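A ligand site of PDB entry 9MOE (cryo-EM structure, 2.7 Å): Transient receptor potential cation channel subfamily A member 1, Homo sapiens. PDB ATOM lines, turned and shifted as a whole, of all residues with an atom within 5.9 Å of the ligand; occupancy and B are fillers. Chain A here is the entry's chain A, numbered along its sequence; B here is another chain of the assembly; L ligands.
N10 of the ligand lies within hydrogen-bond range of NH2 of Arg 853, at 3.5 Å. N of Glu 855 lies within hydrogen-bond range of O3 of the ligand. SG of Cys 857 is in hydrogen-bond range of N8 of the ligand (3.8 Å). The indole nitrogen of Trp 712 sits at hydrogen-bond distance from an oxygen (O2) of the ligand (3.0 Å). The side-chain amide nitrogen of Asn 856 is in hydrogen-bond range of a nitrogen (N8) of the ligand (3.3 Å).
ND1 of His 984 is in hydrogen-bond range of O of Gln 980, 2.9 Å away. The side-chain carboxylate (OE2) of Glu 855 lies close to the side-chain amide oxygen (OE1) of Gln 980 (3.0 Å). SG of Cys 857 sits at hydrogen-bond distance from ND2 of Asn 856, at 3.3 Å. NE2 of His 984 sits close to N of Trp 712, 3.4 Å away. N of Phe 717 lies within hydrogen-bond range of O of Trp 712 (2.9 Å).
OE1 of Gln 980 lies close to N1 of the ligand (3.3 Å). Merely in contact with the ligand: Leu 708 (3.6 Å), Leu 709 (3.9 Å), Phe 717 (3.4 Å), Leu 851 (3.2 Å), Gln 852 (3.9 Å), Phe 854 (3.5 Å), Arg 976 (3.5 Å), Met 979 (3.9 Å), Leu 983 (3.9 Å), His 984 (3.1 Å), Val 876 of chain B (3.6 Å) and Phe 880 of chain B (3.8 Å). Along chain A the residues within 4 Å of the ligand span positions 708 to 984.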
ATOM      1  N   LEU A 708       1.805  -6.278 -24.137  1.00  0.00           N
ATOM      2  CA  LEU A 708       0.917  -7.371 -23.725  1.00  0.00           C
ATOM      3  C   LEU A 708      -0.127  -6.895 -22.723  1.00  0.00           C
ATOM      4  O   LEU A 708      -1.281  -7.308 -22.786  1.00  0.00           O
ATOM      5  CB  LEU A 708       1.735  -8.519 -23.152  1.00  0.00           C
ATOM      6  CG  LEU A 708       1.961  -9.702 -24.098  1.00  0.00           C
ATOM      7  CD1 LEU A 708       2.624 -10.854 -23.373  1.00  0.00           C
ATOM      8  CD2 LEU A 708       0.650 -10.140 -24.719  1.00  0.00           C
ATOM      9  N   LEU A 709       0.276  -6.026 -21.787  1.00  0.00           N
ATOM     10  CA  LEU A 709      -0.689  -5.483 -20.832  1.00  0.00           C
ATOM     11  C   LEU A 709      -1.733  -4.615 -21.518  1.00  0.00           C
ATOM     12  O   LEU A 709      -2.909  -4.619 -21.134  1.00  0.00           O
ATOM     13  CB  LEU A 709       0.043  -4.686 -19.752  1.00  0.00           C
ATOM     14  CG  LEU A 709      -0.827  -4.158 -18.602  1.00  0.00           C
ATOM     15  CD1 LEU A 709      -1.678  -5.267 -18.010  1.00  0.00           C
ATOM     16  CD2 LEU A 709       0.051  -3.526 -17.533  1.00  0.00           C
ATOM     17  N   TRP A 712      -4.139  -6.999 -23.173  1.00  0.00           N
ATOM     18  CA  TRP A 712      -4.958  -7.542 -22.101  1.00  0.00           C
ATOM     19  C   TRP A 712      -6.076  -6.582 -21.753  1.00  0.00           C
ATOM     20  O   TRP A 712      -7.248  -6.861 -22.026  1.00  0.00           O
ATOM     21  CB  TRP A 712      -4.080  -7.826 -20.884  1.00  0.00           C
ATOM     22  CG  TRP A 712      -4.747  -8.523 -19.727  1.00  0.00           C
ATOM     23  CD1 TRP A 712      -4.782  -8.099 -18.426  1.00  0.00           C
ATOM     24  CD2 TRP A 712      -5.448  -9.777 -19.756  1.00  0.00           C
ATOM     25  NE1 TRP A 712      -5.467  -8.997 -17.654  1.00  0.00           N
ATOM     26  CE2 TRP A 712      -5.899 -10.035 -18.439  1.00  0.00           C
ATOM     27  CE3 TRP A 712      -5.761 -10.700 -20.758  1.00  0.00           C
ATOM     28  CZ2 TRP A 712      -6.624 -11.174 -18.105  1.00  0.00           C
ATOM     29  CZ3 TRP A 712      -6.483 -11.822 -20.425  1.00  0.00           C
ATOM     30  CH2 TRP A 712      -6.912 -12.049 -19.114  1.00  0.00           C
ATOM     31  N   PHE A 717      -8.705  -9.312 -21.282  1.00  0.00           N
ATOM     32  CA  PHE A 717      -9.332  -9.452 -19.972  1.00  0.00           C
ATOM     33  C   PHE A 717     -10.845  -9.474 -20.097  1.00  0.00           C
ATOM     34  O   PHE A 717     -11.509 -10.290 -19.461  1.00  0.00           O
ATOM     35  CB  PHE A 717      -8.872  -8.319 -19.059  1.00  0.00           C
ATOM     36  CG  PHE A 717      -9.539  -8.319 -17.717  1.00  0.00           C
ATOM     37  CD1 PHE A 717      -9.121  -9.169 -16.721  1.00  0.00           C
ATOM     38  CD2 PHE A 717     -10.579  -7.441 -17.449  1.00  0.00           C
ATOM     39  CE1 PHE A 717      -9.727  -9.165 -15.488  1.00  0.00           C
ATOM     40  CE2 PHE A 717     -11.191  -7.429 -16.219  1.00  0.00           C
ATOM     41  CZ  PHE A 717     -10.763  -8.300 -15.226  1.00  0.00           C
ATOM     42  N   MET A 721     -13.134 -12.645 -19.174  1.00  0.00           N
ATOM     43  CA  MET A 721     -14.073 -12.461 -18.083  1.00  0.00           C
ATOM     44  C   MET A 721     -15.506 -12.756 -18.531  1.00  0.00           C
ATOM     45  O   MET A 721     -16.307 -13.272 -17.752  1.00  0.00           O
ATOM     46  CB  MET A 721     -13.958 -11.051 -17.524  1.00  0.00           C
ATOM     47  CG  MET A 721     -12.771 -10.863 -16.583  1.00  0.00           C
ATOM     48  SD  MET A 721     -12.644 -12.087 -15.274  1.00  0.00           S
ATOM     49  CE  MET A 721     -14.282 -12.044 -14.558  1.00  0.00           C
ATOM     50  N   PHE A 847     -13.425 -26.025 -14.228  1.00  0.00           N
ATOM     51  CA  PHE A 847     -13.136 -24.662 -13.818  1.00  0.00           C
ATOM     52  C   PHE A 847     -11.636 -24.403 -13.730  1.00  0.00           C
ATOM     53  O   PHE A 847     -11.193 -23.265 -13.857  1.00  0.00           O
ATOM     54  CB  PHE A 847     -13.815 -24.368 -12.475  1.00  0.00           C
ATOM     55  CG  PHE A 847     -13.639 -22.958 -11.996  1.00  0.00           C
ATOM     56  CD1 PHE A 847     -14.145 -21.901 -12.722  1.00  0.00           C
ATOM     57  CD2 PHE A 847     -12.970 -22.693 -10.814  1.00  0.00           C
ATOM     58  CE1 PHE A 847     -13.991 -20.607 -12.279  1.00  0.00           C
ATOM     59  CE2 PHE A 847     -12.810 -21.406 -10.369  1.00  0.00           C
ATOM     60  CZ  PHE A 847     -13.319 -20.354 -11.102  1.00  0.00           C
ATOM     61  N   LEU A 851      -9.007 -21.252 -15.240  1.00  0.00           N
ATOM     62  CA  LEU A 851      -7.951 -20.605 -14.473  1.00  0.00           C
ATOM     63  C   LEU A 851      -6.604 -20.664 -15.166  1.00  0.00           C
ATOM     64  O   LEU A 851      -5.689 -19.946 -14.758  1.00  0.00           O
ATOM     65  CB  LEU A 851      -7.843 -21.240 -13.088  1.00  0.00           C
ATOM     66  CG  LEU A 851      -9.093 -21.199 -12.215  1.00  0.00           C
ATOM     67  CD1 LEU A 851      -8.751 -21.708 -10.829  1.00  0.00           C
ATOM     68  CD2 LEU A 851      -9.669 -19.797 -12.146  1.00  0.00           C
ATOM     69  N   GLN A 852      -6.451 -21.508 -16.183  1.00  0.00           N
ATOM     70  CA  GLN A 852      -5.190 -21.584 -16.904  1.00  0.00           C
ATOM     71  C   GLN A 852      -4.888 -20.309 -17.677  1.00  0.00           C
ATOM     72  O   GLN A 852      -3.750 -20.103 -18.101  1.00  0.00           O
ATOM     73  CB  GLN A 852      -5.211 -22.783 -17.859  1.00  0.00           C
ATOM     74  CG  GLN A 852      -3.850 -23.394 -18.098  1.00  0.00           C
ATOM     75  CD  GLN A 852      -3.882 -24.511 -19.109  1.00  0.00           C
ATOM     76  OE1 GLN A 852      -4.940 -24.813 -19.667  1.00  0.00           O
ATOM     77  NE2 GLN A 852      -2.735 -25.122 -19.358  1.00  0.00           N
ATOM     78  N   ARG A 853      -5.890 -19.441 -17.868  1.00  0.00           N
ATOM     79  CA  ARG A 853      -5.723 -18.179 -18.571  1.00  0.00           C
ATOM     80  C   ARG A 853      -5.480 -17.019 -17.620  1.00  0.00           C
ATOM     81  O   ARG A 853      -5.939 -15.898 -17.872  1.00  0.00           O
ATOM     82  CB  ARG A 853      -6.942 -17.906 -19.455  1.00  0.00           C
ATOM     83  CG  ARG A 853      -7.470 -19.154 -20.159  1.00  0.00           C
ATOM     84  CD  ARG A 853      -7.033 -19.204 -21.613  1.00  0.00           C
ATOM     85  NE  ARG A 853      -5.625 -18.861 -21.771  1.00  0.00           N
ATOM     86  CZ  ARG A 853      -4.629 -19.748 -21.748  1.00  0.00           C
ATOM     87  NH1 ARG A 853      -4.870 -21.043 -21.596  1.00  0.00           N
ATOM     88  NH2 ARG A 853      -3.382 -19.320 -21.883  1.00  0.00           N
ATOM     89  N   PHE A 854      -4.783 -17.268 -16.520  1.00  0.00           N
ATOM     90  CA  PHE A 854      -4.363 -16.232 -15.584  1.00  0.00           C
ATOM     91  C   PHE A 854      -2.881 -16.402 -15.290  1.00  0.00           C
ATOM     92  O   PHE A 854      -2.340 -17.506 -15.365  1.00  0.00           O
ATOM     93  CB  PHE A 854      -5.155 -16.300 -14.280  1.00  0.00           C
ATOM     94  CG  PHE A 854      -6.578 -15.844 -14.414  1.00  0.00           C
ATOM     95  CD1 PHE A 854      -6.881 -14.643 -15.046  1.00  0.00           C
ATOM     96  CD2 PHE A 854      -7.619 -16.601 -13.918  1.00  0.00           C
ATOM     97  CE1 PHE A 854      -8.192 -14.224 -15.177  1.00  0.00           C
ATOM     98  CE2 PHE A 854      -8.930 -16.193 -14.040  1.00  0.00           C
ATOM     99  CZ  PHE A 854      -9.210 -14.997 -14.666  1.00  0.00           C
ATOM    100  N   GLU A 855      -2.227 -15.287 -14.979  1.00  0.00           N
ATOM    101  CA  GLU A 855      -0.779 -15.296 -14.816  1.00  0.00           C
ATOM    102  C   GLU A 855      -0.341 -16.184 -13.657  1.00  0.00           C
ATOM    103  O   GLU A 855       0.627 -16.936 -13.773  1.00  0.00           O
ATOM    104  CB  GLU A 855      -0.265 -13.871 -14.605  1.00  0.00           C
ATOM    105  CG  GLU A 855       0.675 -13.385 -15.676  1.00  0.00           C
ATOM    106  CD  GLU A 855       1.174 -11.983 -15.415  1.00  0.00           C
ATOM    107  OE1 GLU A 855       0.898 -11.456 -14.319  1.00  0.00           O
ATOM    108  OE2 GLU A 855       1.818 -11.396 -16.308  1.00  0.00           O
ATOM    109  N   ASN A 856      -1.046 -16.098 -12.532  1.00  0.00           N
ATOM    110  CA  ASN A 856      -0.637 -16.816 -11.326  1.00  0.00           C
ATOM    111  C   ASN A 856      -1.027 -18.288 -11.346  1.00  0.00           C
ATOM    112  O   ASN A 856      -0.498 -19.061 -10.537  1.00  0.00           O
ATOM    113  CB  ASN A 856      -1.231 -16.139 -10.093  1.00  0.00           C
ATOM    114  CG  ASN A 856      -2.736 -15.976 -10.186  1.00  0.00           C
ATOM    115  OD1 ASN A 856      -3.243 -15.448 -11.167  1.00  0.00           O
ATOM    116  ND2 ASN A 856      -3.442 -16.435  -9.161  1.00  0.00           N
ATOM    117  N   CYS A 857      -1.924 -18.699 -12.240  1.00  0.00           N
ATOM    118  CA  CYS A 857      -2.462 -20.052 -12.215  1.00  0.00           C
ATOM    119  C   CYS A 857      -2.050 -20.905 -13.408  1.00  0.00           C
ATOM    120  O   CYS A 857      -2.132 -22.132 -13.312  1.00  0.00           O
ATOM    121  CB  CYS A 857      -3.992 -20.011 -12.154  1.00  0.00           C
ATOM    122  SG  CYS A 857      -4.682 -19.017 -10.835  1.00  0.00           S
ATOM    123  N   GLY A 858      -1.610 -20.308 -14.509  1.00  0.00           N
ATOM    124  CA  GLY A 858      -1.392 -21.066 -15.726  1.00  0.00           C
ATOM    125  C   GLY A 858      -0.295 -22.107 -15.608  1.00  0.00           C
ATOM    126  O   GLY A 858      -0.450 -23.241 -16.062  1.00  0.00           O
ATOM    127  N   LYS A 975       7.067 -20.020 -21.057  1.00  0.00           N
ATOM    128  CA  LYS A 975       5.761 -20.648 -21.236  1.00  0.00           C
ATOM    129  C   LYS A 975       4.631 -19.718 -20.822  1.00  0.00           C
ATOM    130  O   LYS A 975       3.576 -19.688 -21.468  1.00  0.00           O
ATOM    131  CB  LYS A 975       5.722 -21.965 -20.458  1.00  0.00           C
ATOM    132  CG  LYS A 975       4.419 -22.739 -20.584  1.00  0.00           C
ATOM    133  CD  LYS A 975       4.225 -23.278 -21.989  1.00  0.00           C
ATOM    134  CE  LYS A 975       3.224 -24.410 -22.012  1.00  0.00           C
ATOM    135  NZ  LYS A 975       1.816 -23.918 -21.956  1.00  0.00           N
ATOM    136  N   ARG A 976       4.829 -18.955 -19.743  1.00  0.00           N
ATOM    137  CA  ARG A 976       3.816 -17.996 -19.309  1.00  0.00           C
ATOM    138  C   ARG A 976       3.592 -16.908 -20.355  1.00  0.00           C
ATOM    139  O   ARG A 976       2.451 -16.619 -20.744  1.00  0.00           O
ATOM    140  CB  ARG A 976       4.232 -17.393 -17.972  1.00  0.00           C
ATOM    141  CG  ARG A 976       3.091 -17.117 -17.016  1.00  0.00           C
ATOM    142  CD  ARG A 976       3.604 -16.439 -15.752  1.00  0.00           C
ATOM    143  NE  ARG A 976       4.099 -17.409 -14.782  1.00  0.00           N
ATOM    144  CZ  ARG A 976       5.374 -17.623 -14.522  1.00  0.00           C
ATOM    145  NH1 ARG A 976       6.330 -16.936 -15.127  1.00  0.00           N
ATOM    146  NH2 ARG A 976       5.714 -18.551 -13.633  1.00  0.00           N
ATOM    147  N   ILE A 977       4.688 -16.298 -20.821  1.00  0.00           N
ATOM    148  CA  ILE A 977       4.542 -15.249 -21.821  1.00  0.00           C
ATOM    149  C   ILE A 977       3.993 -15.820 -23.122  1.00  0.00           C
ATOM    150  O   ILE A 977       3.206 -15.154 -23.816  1.00  0.00           O
ATOM    151  CB  ILE A 977       5.882 -14.514 -22.027  1.00  0.00           C
ATOM    152  CG1 ILE A 977       6.309 -13.820 -20.735  1.00  0.00           C
ATOM    153  CG2 ILE A 977       5.768 -13.489 -23.141  1.00  0.00           C
ATOM    154  CD1 ILE A 977       7.674 -13.207 -20.795  1.00  0.00           C
ATOM    155  N   MET A 979       1.879 -18.336 -23.330  1.00  0.00           N
ATOM    156  CA  MET A 979       0.448 -18.517 -23.122  1.00  0.00           C
ATOM    157  C   MET A 979      -0.301 -17.203 -23.308  1.00  0.00           C
ATOM    158  O   MET A 979      -1.366 -17.175 -23.934  1.00  0.00           O
ATOM    159  CB  MET A 979       0.168 -19.082 -21.735  1.00  0.00           C
ATOM    160  CG  MET A 979       0.459 -20.560 -21.566  1.00  0.00           C
ATOM    161  SD  MET A 979       0.085 -21.141 -19.900  1.00  0.00           S
ATOM    162  CE  MET A 979       1.674 -20.963 -19.105  1.00  0.00           C
ATOM    163  N   GLN A 980       0.229 -16.107 -22.769  1.00  0.00           N
ATOM    164  CA  GLN A 980      -0.420 -14.815 -22.956  1.00  0.00           C
ATOM    165  C   GLN A 980      -0.455 -14.421 -24.433  1.00  0.00           C
ATOM    166  O   GLN A 980      -1.486 -13.969 -24.952  1.00  0.00           O
ATOM    167  CB  GLN A 980       0.272 -13.739 -22.131  1.00  0.00           C
ATOM    168  CG  GLN A 980       0.441 -14.105 -20.682  1.00  0.00           C
ATOM    169  CD  GLN A 980       1.128 -13.018 -19.889  1.00  0.00           C
ATOM    170  OE1 GLN A 980       0.739 -12.707 -18.768  1.00  0.00           O
ATOM    171  NE2 GLN A 980       2.175 -12.433 -20.460  1.00  0.00           N
ATOM    172  N   LEU A 983      -2.995 -16.589 -26.279  1.00  0.00           N
ATOM    173  CA  LEU A 983      -4.355 -16.188 -25.965  1.00  0.00           C
ATOM    174  C   LEU A 983      -4.759 -14.968 -26.764  1.00  0.00           C
ATOM    175  O   LEU A 983      -5.821 -14.942 -27.404  1.00  0.00           O
ATOM    176  CB  LEU A 983      -4.487 -15.920 -24.466  1.00  0.00           C
ATOM    177  CG  LEU A 983      -5.704 -15.110 -24.016  1.00  0.00           C
ATOM    178  CD1 LEU A 983      -6.908 -16.007 -23.831  1.00  0.00           C
ATOM    179  CD2 LEU A 983      -5.402 -14.342 -22.749  1.00  0.00           C
ATOM    180  N   HIS A 984      -3.910 -13.938 -26.768  1.00  0.00           N
ATOM    181  CA  HIS A 984      -4.282 -12.715 -27.478  1.00  0.00           C
ATOM    182  C   HIS A 984      -4.244 -12.891 -28.990  1.00  0.00           C
ATOM    183  O   HIS A 984      -5.059 -12.296 -29.698  1.00  0.00           O
ATOM    184  CB  HIS A 984      -3.386 -11.570 -27.021  1.00  0.00           C
ATOM    185  CG  HIS A 984      -3.645 -11.141 -25.609  1.00  0.00           C
ATOM    186  ND1 HIS A 984      -2.743 -11.347 -24.593  1.00  0.00           N
ATOM    187  CD2 HIS A 984      -4.716 -10.547 -25.038  1.00  0.00           C
ATOM    188  CE1 HIS A 984      -3.245 -10.886 -23.466  1.00  0.00           C
ATOM    189  NE2 HIS A 984      -4.438 -10.387 -23.709  1.00  0.00           N
ATOM    190  N   VAL B 876      -4.428 -21.575  -3.947  1.00  0.00           N
ATOM    191  CA  VAL B 876      -5.497 -20.861  -4.616  1.00  0.00           C
ATOM    192  C   VAL B 876      -5.933 -21.546  -5.897  1.00  0.00           C
ATOM    193  O   VAL B 876      -6.963 -21.180  -6.471  1.00  0.00           O
ATOM    194  CB  VAL B 876      -5.080 -19.400  -4.903  1.00  0.00           C
ATOM    195  CG1 VAL B 876      -4.932 -18.631  -3.595  1.00  0.00           C
ATOM    196  CG2 VAL B 876      -3.779 -19.365  -5.685  1.00  0.00           C
ATOM    197  N   VAL B 877      -5.177 -22.525  -6.371  1.00  0.00           N
ATOM    198  CA  VAL B 877      -5.517 -23.297  -7.552  1.00  0.00           C
ATOM    199  C   VAL B 877      -6.128 -24.645  -7.195  1.00  0.00           C
ATOM    200  O   VAL B 877      -7.186 -25.009  -7.694  1.00  0.00           O
ATOM    201  CB  VAL B 877      -4.273 -23.463  -8.450  1.00  0.00           C
ATOM    202  CG1 VAL B 877      -4.691 -23.792  -9.869  1.00  0.00           C
ATOM    203  CG2 VAL B 877      -3.435 -22.198  -8.424  1.00  0.00           C
ATOM    204  N   PHE B 880      -9.829 -25.599  -5.597  1.00  0.00           N
ATOM    205  CA  PHE B 880     -10.980 -25.960  -6.414  1.00  0.00           C
ATOM    206  C   PHE B 880     -11.016 -27.440  -6.732  1.00  0.00           C
ATOM    207  O   PHE B 880     -12.108 -28.017  -6.834  1.00  0.00           O
ATOM    208  CB  PHE B 880     -10.974 -25.121  -7.697  1.00  0.00           C
ATOM    209  CG  PHE B 880     -11.014 -23.645  -7.434  1.00  0.00           C
ATOM    210  CD1 PHE B 880     -12.135 -23.069  -6.867  1.00  0.00           C
ATOM    211  CD2 PHE B 880      -9.928 -22.845  -7.719  1.00  0.00           C
ATOM    212  CE1 PHE B 880     -12.185 -21.716  -6.615  1.00  0.00           C
ATOM    213  CE2 PHE B 880      -9.970 -21.488  -7.472  1.00  0.00           C
ATOM    214  CZ  PHE B 880     -11.093 -20.930  -6.918  1.00  0.00           C
HETATM  215  O1  LIG L   1      -2.509 -12.106 -20.689  1.00  0.00           O
HETATM  216  C1  LIG L   1      -2.009  -9.710 -13.274  1.00  0.00           C
HETATM  217  O2  LIG L   1      -4.840  -9.699 -14.854  1.00  0.00           O
HETATM  218  C2  LIG L   1      -2.671 -10.597 -14.318  1.00  0.00           C
HETATM  219  C3  LIG L   1      -2.490 -11.737 -19.530  1.00  0.00           C
HETATM  220  N1  LIG L   1      -1.803 -10.596 -19.147  1.00  0.00           N
HETATM  221  C4  LIG L   1      -1.440  -9.176 -16.038  1.00  0.00           C
HETATM  222  C5  LIG L   1      -2.434 -10.925 -16.877  1.00  0.00           C
HETATM  223  C6  LIG L   1      -1.792 -10.211 -17.838  1.00  0.00           C
HETATM  224  C7  LIG L   1      -1.119  -9.812 -20.178  1.00  0.00           C
HETATM  225  N2  LIG L   1      -3.119 -12.451 -18.522  1.00  0.00           N
HETATM  226  C8  LIG L   1      -3.154 -12.118 -17.167  1.00  0.00           C
HETATM  227  O3  LIG L   1      -3.756 -12.827 -16.374  1.00  0.00           O
HETATM  228  C9  LIG L   1      -7.133 -10.888 -13.569  1.00  0.00           C
HETATM  229  C10 LIG L   1      -8.408 -11.205 -13.160  1.00  0.00           C
HETATM  230  C11 LIG L   1      -8.614 -12.229 -12.259  1.00  0.00           C
HETATM  231  C12 LIG L   1      -7.512 -12.936 -11.782  1.00  0.00           C
HETATM  232  C13 LIG L   1      -7.658 -14.046 -10.805  1.00  0.00           C
HETATM  233  C14 LIG L   1      -8.897 -14.599 -10.528  1.00  0.00           C
HETATM  234  C15 LIG L   1      -7.927 -16.382  -9.580  1.00  0.00           C
HETATM  235  C16 LIG L   1      -6.570 -14.809 -10.412  1.00  0.00           C
HETATM  236  C17 LIG L   1      -8.042 -17.721  -8.870  1.00  0.00           C
HETATM  237  C18 LIG L   1      -3.854 -13.657 -18.888  1.00  0.00           C
HETATM  238  C19 LIG L   1      -2.962 -14.849 -19.003  1.00  0.00           C
HETATM  239  C20 LIG L   1      -1.496 -16.323 -18.889  1.00  0.00           C
HETATM  240  C21 LIG L   1      -0.243 -17.004 -18.486  1.00  0.00           C
HETATM  241  C22 LIG L   1      -4.197 -10.525 -14.215  1.00  0.00           C
HETATM  242  C23 LIG L   1      -6.077 -11.648 -13.046  1.00  0.00           C
HETATM  243  F1  LIG L   1      -7.873 -18.737  -9.703  1.00  0.00           F
HETATM  244  F2  LIG L   1      -9.234 -17.871  -8.305  1.00  0.00           F
HETATM  245  F3  LIG L   1      -7.144 -17.852  -7.908  1.00  0.00           F
HETATM  246  N3  LIG L   1      -2.204 -10.246 -15.685  1.00  0.00           N
HETATM  247  N4  LIG L   1      -1.172  -9.113 -17.327  1.00  0.00           N
HETATM  248  N5  LIG L   1      -4.723 -11.438 -13.371  1.00  0.00           N
HETATM  249  N6  LIG L   1      -6.258 -12.642 -12.164  1.00  0.00           N
HETATM  250  N7  LIG L   1      -9.070 -15.769  -9.904  1.00  0.00           N
HETATM  251  N8  LIG L   1      -6.663 -15.992  -9.788  1.00  0.00           N
HETATM  252  N9  LIG L   1      -1.828 -15.078 -18.417  1.00  0.00           N
HETATM  253  N10 LIG L   1      -2.361 -16.844 -19.703  1.00  0.00           N
HETATM  254  O4  LIG L   1      -3.370 -15.850 -19.786  1.00  0.00           O
